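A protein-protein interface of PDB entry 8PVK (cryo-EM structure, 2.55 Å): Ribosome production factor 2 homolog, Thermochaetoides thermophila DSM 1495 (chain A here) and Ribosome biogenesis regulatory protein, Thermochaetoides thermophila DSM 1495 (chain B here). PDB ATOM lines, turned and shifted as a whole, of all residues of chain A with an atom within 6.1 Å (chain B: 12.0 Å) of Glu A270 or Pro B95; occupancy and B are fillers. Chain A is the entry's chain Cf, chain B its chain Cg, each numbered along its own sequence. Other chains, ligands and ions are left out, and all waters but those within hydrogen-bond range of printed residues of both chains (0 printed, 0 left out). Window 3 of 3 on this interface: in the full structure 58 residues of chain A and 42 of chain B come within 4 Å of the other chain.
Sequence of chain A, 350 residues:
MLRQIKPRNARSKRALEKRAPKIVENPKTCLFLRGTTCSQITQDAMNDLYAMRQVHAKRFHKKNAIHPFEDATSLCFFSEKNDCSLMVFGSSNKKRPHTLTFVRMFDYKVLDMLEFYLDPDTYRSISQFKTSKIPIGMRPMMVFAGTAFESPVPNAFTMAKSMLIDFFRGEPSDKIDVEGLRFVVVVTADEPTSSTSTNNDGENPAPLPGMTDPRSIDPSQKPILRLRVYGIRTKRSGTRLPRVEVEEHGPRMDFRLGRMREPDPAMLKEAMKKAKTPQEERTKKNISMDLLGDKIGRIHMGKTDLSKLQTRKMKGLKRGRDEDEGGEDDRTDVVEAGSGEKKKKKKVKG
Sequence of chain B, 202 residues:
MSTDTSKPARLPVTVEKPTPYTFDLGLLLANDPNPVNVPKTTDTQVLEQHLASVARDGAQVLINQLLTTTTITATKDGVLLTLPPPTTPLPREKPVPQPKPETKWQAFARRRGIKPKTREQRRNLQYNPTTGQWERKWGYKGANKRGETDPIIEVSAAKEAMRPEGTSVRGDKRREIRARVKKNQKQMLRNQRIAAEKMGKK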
ATOM      1  N   PRO A  21       5.694  -8.881  29.476  1.00  0.00           N
ATOM      2  CA  PRO A  21       6.181  -9.453  28.214  1.00  0.00           C
ATOM      3  C   PRO A  21       7.037 -10.688  28.458  1.00  0.00           C
ATOM      4  O   PRO A  21       7.770 -10.775  29.445  1.00  0.00           O
ATOM      5  CB  PRO A  21       7.000  -8.313  27.598  1.00  0.00           C
ATOM      6  CG  PRO A  21       6.488  -7.076  28.255  1.00  0.00           C
ATOM      7  CD  PRO A  21       6.136  -7.487  29.649  1.00  0.00           C
ATOM      8  N   LYS A  22       6.937 -11.650  27.543  1.00  0.00           N
ATOM      9  CA  LYS A  22       7.582 -12.944  27.692  1.00  0.00           C
ATOM     10  C   LYS A  22       8.261 -13.340  26.389  1.00  0.00           C
ATOM     11  O   LYS A  22       7.917 -12.851  25.310  1.00  0.00           O
ATOM     12  CB  LYS A  22       6.576 -14.032  28.101  1.00  0.00           C
ATOM     13  CG  LYS A  22       5.964 -13.836  29.480  1.00  0.00           C
ATOM     14  CD  LYS A  22       4.796 -14.779  29.709  1.00  0.00           C
ATOM     15  CE  LYS A  22       4.159 -14.542  31.069  1.00  0.00           C
ATOM     16  NZ  LYS A  22       3.021 -15.467  31.320  1.00  0.00           N
ATOM     17  N   GLU A  25       5.039 -16.140  24.239  1.00  0.00           N
ATOM     18  CA  GLU A  25       3.863 -15.368  24.597  1.00  0.00           C
ATOM     19  C   GLU A  25       2.709 -16.277  25.009  1.00  0.00           C
ATOM     20  O   GLU A  25       2.642 -17.454  24.646  1.00  0.00           O
ATOM     21  CB  GLU A  25       3.435 -14.473  23.433  1.00  0.00           C
ATOM     22  CG  GLU A  25       4.333 -13.267  23.224  1.00  0.00           C
ATOM     23  CD  GLU A  25       3.746 -12.262  22.257  1.00  0.00           C
ATOM     24  OE1 GLU A  25       2.969 -12.673  21.369  1.00  0.00           O
ATOM     25  OE2 GLU A  25       4.059 -11.060  22.384  1.00  0.00           O
ATOM     26  N   PHE A 106      -0.617  -4.253  19.255  1.00  0.00           N
ATOM     27  CA  PHE A 106       0.781  -4.566  19.546  1.00  0.00           C
ATOM     28  C   PHE A 106       1.256  -3.569  20.589  1.00  0.00           C
ATOM     29  O   PHE A 106       1.277  -2.365  20.313  1.00  0.00           O
ATOM     30  CB  PHE A 106       1.662  -4.495  18.301  1.00  0.00           C
ATOM     31  CG  PHE A 106       3.129  -4.653  18.596  1.00  0.00           C
ATOM     32  CD1 PHE A 106       3.642  -5.877  18.984  1.00  0.00           C
ATOM     33  CD2 PHE A 106       3.991  -3.575  18.494  1.00  0.00           C
ATOM     34  CE1 PHE A 106       4.986  -6.030  19.263  1.00  0.00           C
ATOM     35  CE2 PHE A 106       5.341  -3.721  18.769  1.00  0.00           C
ATOM     36  CZ  PHE A 106       5.835  -4.952  19.152  1.00  0.00           C
ATOM     37  N   ASP A 107       1.641  -4.072  21.768  1.00  0.00           N
ATOM     38  CA  ASP A 107       2.061  -3.253  22.911  1.00  0.00           C
ATOM     39  C   ASP A 107       0.993  -2.226  23.287  1.00  0.00           C
ATOM     40  O   ASP A 107       1.287  -1.046  23.496  1.00  0.00           O
ATOM     41  CB  ASP A 107       3.411  -2.577  22.652  1.00  0.00           C
ATOM     42  CG  ASP A 107       4.101  -2.136  23.931  1.00  0.00           C
ATOM     43  OD1 ASP A 107       4.193  -2.951  24.873  1.00  0.00           O
ATOM     44  OD2 ASP A 107       4.547  -0.971  23.993  1.00  0.00           O
ATOM     45  N   PRO A 265       5.788   0.483   9.385  1.00  0.00           N
ATOM     46  CA  PRO A 265       6.849  -0.502   9.089  1.00  0.00           C
ATOM     47  C   PRO A 265       7.745  -0.840  10.272  1.00  0.00           C
ATOM     48  O   PRO A 265       8.088  -2.014  10.461  1.00  0.00           O
ATOM     49  CB  PRO A 265       7.636   0.174   7.958  1.00  0.00           C
ATOM     50  CG  PRO A 265       6.645   1.069   7.300  1.00  0.00           C
ATOM     51  CD  PRO A 265       5.763   1.579   8.401  1.00  0.00           C
ATOM     52  N   ALA A 266       8.115   0.150  11.091  1.00  0.00           N
ATOM     53  CA  ALA A 266       8.971  -0.125  12.243  1.00  0.00           C
ATOM     54  C   ALA A 266       8.233  -0.935  13.302  1.00  0.00           C
ATOM     55  O   ALA A 266       8.799  -1.869  13.888  1.00  0.00           O
ATOM     56  CB  ALA A 266       9.496   1.182  12.833  1.00  0.00           C
ATOM     57  N   MET A 267       6.967  -0.593  13.556  1.00  0.00           N
ATOM     58  CA  MET A 267       6.158  -1.354  14.503  1.00  0.00           C
ATOM     59  C   MET A 267       5.931  -2.777  14.007  1.00  0.00           C
ATOM     60  O   MET A 267       5.955  -3.727  14.798  1.00  0.00           O
ATOM     61  CB  MET A 267       4.828  -0.637  14.741  1.00  0.00           C
ATOM     62  CG  MET A 267       3.828  -1.410  15.586  1.00  0.00           C
ATOM     63  SD  MET A 267       2.312  -0.488  15.902  1.00  0.00           S
ATOM     64  CE  MET A 267       2.705   0.279  17.472  1.00  0.00           C
ATOM     65  N   LEU A 268       5.736  -2.944  12.697  1.00  0.00           N
ATOM     66  CA  LEU A 268       5.572  -4.278  12.129  1.00  0.00           C
ATOM     67  C   LEU A 268       6.853  -5.095  12.246  1.00  0.00           C
ATOM     68  O   LEU A 268       6.799  -6.295  12.532  1.00  0.00           O
ATOM     69  CB  LEU A 268       5.135  -4.176  10.669  1.00  0.00           C
ATOM     70  CG  LEU A 268       4.843  -5.508   9.975  1.00  0.00           C
ATOM     71  CD1 LEU A 268       3.725  -6.246  10.691  1.00  0.00           C
ATOM     72  CD2 LEU A 268       4.500  -5.290   8.512  1.00  0.00           C
ATOM     73  N   LYS A 269       8.011  -4.465  12.028  1.00  0.00           N
ATOM     74  CA  LYS A 269       9.281  -5.166  12.205  1.00  0.00           C
ATOM     75  C   LYS A 269       9.479  -5.590  13.656  1.00  0.00           C
ATOM     76  O   LYS A 269       9.896  -6.725  13.930  1.00  0.00           O
ATOM     77  CB  LYS A 269      10.434  -4.277  11.742  1.00  0.00           C
ATOM     78  CG  LYS A 269      11.811  -4.896  11.911  1.00  0.00           C
ATOM     79  CD  LYS A 269      12.898  -3.960  11.411  1.00  0.00           C
ATOM     80  CE  LYS A 269      14.272  -4.600  11.516  1.00  0.00           C
ATOM     81  NZ  LYS A 269      14.700  -4.771  12.932  1.00  0.00           N
ATOM     82  N   GLU A 270       9.157  -4.698  14.599  1.00  0.00           N
ATOM     83  CA  GLU A 270       9.271  -5.030  16.015  1.00  0.00           C
ATOM     84  C   GLU A 270       8.291  -6.127  16.419  1.00  0.00           C
ATOM     85  O   GLU A 270       8.599  -6.938  17.298  1.00  0.00           O
ATOM     86  CB  GLU A 270       9.057  -3.771  16.859  1.00  0.00           C
ATOM     87  CG  GLU A 270       9.427  -3.917  18.327  1.00  0.00           C
ATOM     88  CD  GLU A 270       8.691  -2.931  19.214  1.00  0.00           C
ATOM     89  OE1 GLU A 270       8.538  -1.761  18.805  1.00  0.00           O
ATOM     90  OE2 GLU A 270       8.275  -3.320  20.325  1.00  0.00           O
ATOM     91  N   ALA A 271       7.117  -6.174  15.785  1.00  0.00           N
ATOM     92  CA  ALA A 271       6.148  -7.224  16.078  1.00  0.00           C
ATOM     93  C   ALA A 271       6.536  -8.563  15.465  1.00  0.00           C
ATOM     94  O   ALA A 271       6.276  -9.610  16.068  1.00  0.00           O
ATOM     95  CB  ALA A 271       4.760  -6.808  15.588  1.00  0.00           C
ATOM     96  N   MET A 272       7.150  -8.559  14.284  1.00  0.00           N
ATOM     97  CA  MET A 272       7.580  -9.790  13.635  1.00  0.00           C
ATOM     98  C   MET A 272       8.992 -10.210  14.019  1.00  0.00           C
ATOM     99  O   MET A 272       9.503 -11.180  13.449  1.00  0.00           O
ATOM    100  CB  MET A 272       7.485  -9.666  12.109  1.00  0.00           C
ATOM    101  CG  MET A 272       6.118  -9.266  11.580  1.00  0.00           C
ATOM    102  SD  MET A 272       4.899 -10.584  11.720  1.00  0.00           S
ATOM    103  CE  MET A 272       4.648 -10.992   9.995  1.00  0.00           C
ATOM    104  N   LYS A 273       9.644  -9.496  14.936  1.00  0.00           N
ATOM    105  CA  LYS A 273      10.846 -10.033  15.562  1.00  0.00           C
ATOM    106  C   LYS A 273      10.527 -11.336  16.290  1.00  0.00           C
ATOM    107  O   LYS A 273       9.507 -11.449  16.976  1.00  0.00           O
ATOM    108  CB  LYS A 273      11.447  -9.027  16.545  1.00  0.00           C
ATOM    109  CG  LYS A 273      12.238  -7.904  15.904  1.00  0.00           C
ATOM    110  CD  LYS A 273      12.819  -6.980  16.963  1.00  0.00           C
ATOM    111  CE  LYS A 273      13.536  -5.796  16.338  1.00  0.00           C
ATOM    112  NZ  LYS A 273      14.026  -4.842  17.371  1.00  0.00           N
ATOM    113  N   PRO B  89       4.489 -16.699   9.536  1.00  0.00           N
ATOM    114  CA  PRO B  89       4.805 -15.509  10.338  1.00  0.00           C
ATOM    115  C   PRO B  89       3.540 -14.788  10.785  1.00  0.00           C
ATOM    116  O   PRO B  89       2.696 -14.418   9.967  1.00  0.00           O
ATOM    117  CB  PRO B  89       5.637 -14.644   9.382  1.00  0.00           C
ATOM    118  CG  PRO B  89       6.053 -15.568   8.269  1.00  0.00           C
ATOM    119  CD  PRO B  89       4.947 -16.561   8.146  1.00  0.00           C
ATOM    120  N   LEU B  90       3.417 -14.597  12.095  1.00  0.00           N
ATOM    121  CA  LEU B  90       2.339 -13.836  12.701  1.00  0.00           C
ATOM    122  C   LEU B  90       2.916 -12.868  13.723  1.00  0.00           C
ATOM    123  O   LEU B  90       3.927 -13.172  14.365  1.00  0.00           O
ATOM    124  CB  LEU B  90       1.312 -14.760  13.374  1.00  0.00           C
ATOM    125  CG  LEU B  90       0.453 -15.593  12.423  1.00  0.00           C
ATOM    126  CD1 LEU B  90      -0.189 -16.745  13.162  1.00  0.00           C
ATOM    127  CD2 LEU B  90      -0.603 -14.729  11.754  1.00  0.00           C
ATOM    128  N   PRO B  91       2.309 -11.692  13.884  1.00  0.00           N
ATOM    129  CA  PRO B  91       2.898 -10.677  14.764  1.00  0.00           C
ATOM    130  C   PRO B  91       2.796 -11.044  16.235  1.00  0.00           C
ATOM    131  O   PRO B  91       1.868 -11.727  16.674  1.00  0.00           O
ATOM    132  CB  PRO B  91       2.074  -9.422  14.457  1.00  0.00           C
ATOM    133  CG  PRO B  91       0.775  -9.944  13.960  1.00  0.00           C
ATOM    134  CD  PRO B  91       1.111 -11.184  13.191  1.00  0.00           C
ATOM    135  N   ARG B  92       3.784 -10.578  16.996  1.00  0.00           N
ATOM    136  CA  ARG B  92       3.708 -10.595  18.446  1.00  0.00           C
ATOM    137  C   ARG B  92       2.846  -9.426  18.918  1.00  0.00           C
ATOM    138  O   ARG B  92       2.389  -8.597  18.127  1.00  0.00           O
ATOM    139  CB  ARG B  92       5.108 -10.535  19.054  1.00  0.00           C
ATOM    140  CG  ARG B  92       5.879 -11.841  18.989  1.00  0.00           C
ATOM    141  CD  ARG B  92       7.312 -11.639  19.446  1.00  0.00           C
ATOM    142  NE  ARG B  92       7.396 -11.043  20.774  1.00  0.00           N
ATOM    143  CZ  ARG B  92       7.572 -11.739  21.888  1.00  0.00           C
ATOM    144  NH1 ARG B  92       7.696 -13.055  21.869  1.00  0.00           N
ATOM    145  NH2 ARG B  92       7.634 -11.096  23.051  1.00  0.00           N
ATOM    146  N   GLU B  93       2.601  -9.370  20.223  1.00  0.00           N
ATOM    147  CA  GLU B  93       1.793  -8.317  20.839  1.00  0.00           C
ATOM    148  C   GLU B  93       2.369  -7.725  22.112  1.00  0.00           C
ATOM    149  O   GLU B  93       1.790  -6.761  22.628  1.00  0.00           O
ATOM    150  CB  GLU B  93       0.368  -8.823  21.086  1.00  0.00           C
ATOM    151  CG  GLU B  93      -0.399  -8.949  19.793  1.00  0.00           C
ATOM    152  CD  GLU B  93      -1.291 -10.145  19.710  1.00  0.00           C
ATOM    153  OE1 GLU B  93      -1.870 -10.589  20.721  1.00  0.00           O
ATOM    154  OE2 GLU B  93      -1.440 -10.623  18.570  1.00  0.00           O
ATOM    155  N   LYS B  94       3.482  -8.242  22.620  1.00  0.00           N
ATOM    156  CA  LYS B  94       4.353  -7.580  23.576  1.00  0.00           C
ATOM    157  C   LYS B  94       5.788  -7.683  23.083  1.00  0.00           C
ATOM    158  O   LYS B  94       6.172  -8.700  22.496  1.00  0.00           O
ATOM    159  CB  LYS B  94       4.229  -8.198  24.977  1.00  0.00           C
ATOM    160  CG  LYS B  94       2.907  -7.887  25.651  1.00  0.00           C
ATOM    161  CD  LYS B  94       2.656  -8.729  26.888  1.00  0.00           C
ATOM    162  CE  LYS B  94       1.223  -8.523  27.354  1.00  0.00           C
ATOM    163  NZ  LYS B  94       0.805  -9.465  28.425  1.00  0.00           N
ATOM    164  N   PRO B  95       6.596  -6.644  23.299  1.00  0.00           N
ATOM    165  CA  PRO B  95       7.945  -6.624  22.721  1.00  0.00           C
ATOM    166  C   PRO B  95       8.835  -7.683  23.344  1.00  0.00           C
ATOM    167  O   PRO B  95       8.600  -8.139  24.465  1.00  0.00           O
ATOM    168  CB  PRO B  95       8.454  -5.214  23.050  1.00  0.00           C
ATOM    169  CG  PRO B  95       7.613  -4.770  24.204  1.00  0.00           C
ATOM    170  CD  PRO B  95       6.272  -5.378  23.976  1.00  0.00           C
ATOM    171  N   VAL B  96       9.841  -8.099  22.577  1.00  0.00           N
ATOM    172  CA  VAL B  96      10.821  -9.055  23.101  1.00  0.00           C
ATOM    173  C   VAL B  96      11.539  -8.417  24.281  1.00  0.00           C
ATOM    174  O   VAL B  96      12.074  -7.299  24.145  1.00  0.00           O
ATOM    175  CB  VAL B  96      11.816  -9.465  22.004  1.00  0.00           C
ATOM    176  CG1 VAL B  96      12.942 -10.300  22.593  1.00  0.00           C
ATOM    177  CG2 VAL B  96      11.102 -10.226  20.900  1.00  0.00           C
ATOM    178  N   PRO B  97      11.539  -9.049  25.456  1.00  0.00           N
ATOM    179  CA  PRO B  97      12.020  -8.371  26.665  1.00  0.00           C
ATOM    180  C   PRO B  97      13.507  -8.065  26.595  1.00  0.00           C
ATOM    181  O   PRO B  97      14.308  -8.864  26.107  1.00  0.00           O
ATOM    182  CB  PRO B  97      11.703  -9.372  27.782  1.00  0.00           C
ATOM    183  CG  PRO B  97      10.653 -10.273  27.206  1.00  0.00           C
ATOM    184  CD  PRO B  97      10.981 -10.377  25.755  1.00  0.00           C
ATOM    185  N   GLN B  98      13.859  -6.888  27.078  1.00  0.00           N
ATOM    186  CA  GLN B  98      15.218  -6.395  27.091  1.00  0.00           C
ATOM    187  C   GLN B  98      15.764  -6.423  28.513  1.00  0.00           C
ATOM    188  O   GLN B  98      14.987  -6.407  29.475  1.00  0.00           O
ATOM    189  CB  GLN B  98      15.283  -4.965  26.541  1.00  0.00           C
ATOM    190  CG  GLN B  98      14.868  -4.847  25.085  1.00  0.00           C
ATOM    191  CD  GLN B  98      15.598  -5.828  24.190  1.00  0.00           C
ATOM    192  OE1 GLN B  98      15.011  -6.789  23.694  1.00  0.00           O
ATOM    193  NE2 GLN B  98      16.889  -5.593  23.983  1.00  0.00           N
ATOM    194  N   PRO B  99      17.083  -6.517  28.682  1.00  0.00           N
ATOM    195  CA  PRO B  99      17.659  -6.406  30.027  1.00  0.00           C
ATOM    196  C   PRO B  99      17.362  -5.047  30.643  1.00  0.00           C
ATOM    197  O   PRO B  99      17.318  -4.026  29.953  1.00  0.00           O
ATOM    198  CB  PRO B  99      19.159  -6.602  29.787  1.00  0.00           C
ATOM    199  CG  PRO B  99      19.233  -7.394  28.529  1.00  0.00           C
ATOM    200  CD  PRO B  99      18.091  -6.920  27.685  1.00  0.00           C
ATOM    201  N   LYS B 100      17.136  -5.051  31.955  1.00  0.00           N
ATOM    202  CA  LYS B 100      16.840  -3.825  32.670  1.00  0.00           C
ATOM    203  C   LYS B 100      18.063  -2.910  32.673  1.00  0.00           C
ATOM    204  O   LYS B 100      19.195  -3.381  32.514  1.00  0.00           O
ATOM    205  CB  LYS B 100      16.415  -4.134  34.105  1.00  0.00           C
ATOM    206  CG  LYS B 100      15.236  -5.084  34.213  1.00  0.00           C
ATOM    207  CD  LYS B 100      14.906  -5.387  35.665  1.00  0.00           C
ATOM    208  CE  LYS B 100      13.770  -6.391  35.772  1.00  0.00           C
ATOM    209  NZ  LYS B 100      13.475  -6.747  37.187  1.00  0.00           N
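SD of Met A272 sits close to N of Pro B91.
O of Ala A271 is in hydrogen-bond range of N of Arg B92.
OE2 of Glu A25 sits at hydrogen-bond distance from N of Lys B94.
The guanidinium group (NH2) of Arg B92 lies within salt-bridge range of the side-chain carboxylate (OE2) of Glu A25, at 3.6 Å.
The backbone carbonyl oxygen (O) of Lys A22 sits at hydrogen-bond distance from the guanidinium group (NH2) of Arg B92, at 2.9 Å.
The backbone carbonyl oxygen (O) of Glu B93 is in hydrogen-bond range of the backbone NH (N) of Asp A107, at 2.8 Å.
OE2 of Glu A25 is in hydrogen-bond range of N of Glu B93, at 3.1 Å.
The backbone carbonyl oxygen of Lys B94 lies within hydrogen-bond range of the guanidinium group of Arg B92 (2.9 Å).
The guanidinium group (NH2) of Arg B92 lies within hydrogen-bond range of the backbone carbonyl oxygen (O) of Pro B95, at 3.4 Å.
Among the printed residues, merely in contact across the chains: Phe A106 with Arg B92, Lys A273 with Arg B92, Asp A107 with Pro B95, Glu A270 with Pro B95, Pro A21 with Pro B95, Phe A106 with Glu B93, Met A272 with Leu B90, Pro A21 with Pro B97, Ala A271 with Pro B91, Pro A21 with Lys B94, Met A272 with Pro B89 and Lys A22 with Pro B97.
Of the printed residues of chain B, Lys A22 touches Arg B92 and Pro B97.
Asp A107 touches just these residues of chain B: Glu B93 (2.8 Å) and Pro B95 (3.3 Å).
No residue of chain B comes within 4 Å of Leu A268.
No residue of chain B comes within 4 Å of Lys A269.
Of the printed residues of chain B, Glu A270 touches Pro B95.
Ala A271 touches two residues of chain B.
Of the printed residues of chain A, Arg B92 touches Lys A22, Glu A25, Phe A106, Ala A271 and Lys A273.
Of the printed residues of chain A, Glu B93 touches Glu A25, Phe A106 and Asp A107.
The nearest printed residue of chain A that does not touch Pro B89 is Ala A271 (7.9 Å).
Along chain B the printed residues that touch a printed residue of chain A span positions 89 to 97.
Of the 14 printed residues of chain A, 9 touch a printed residue of chain B.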
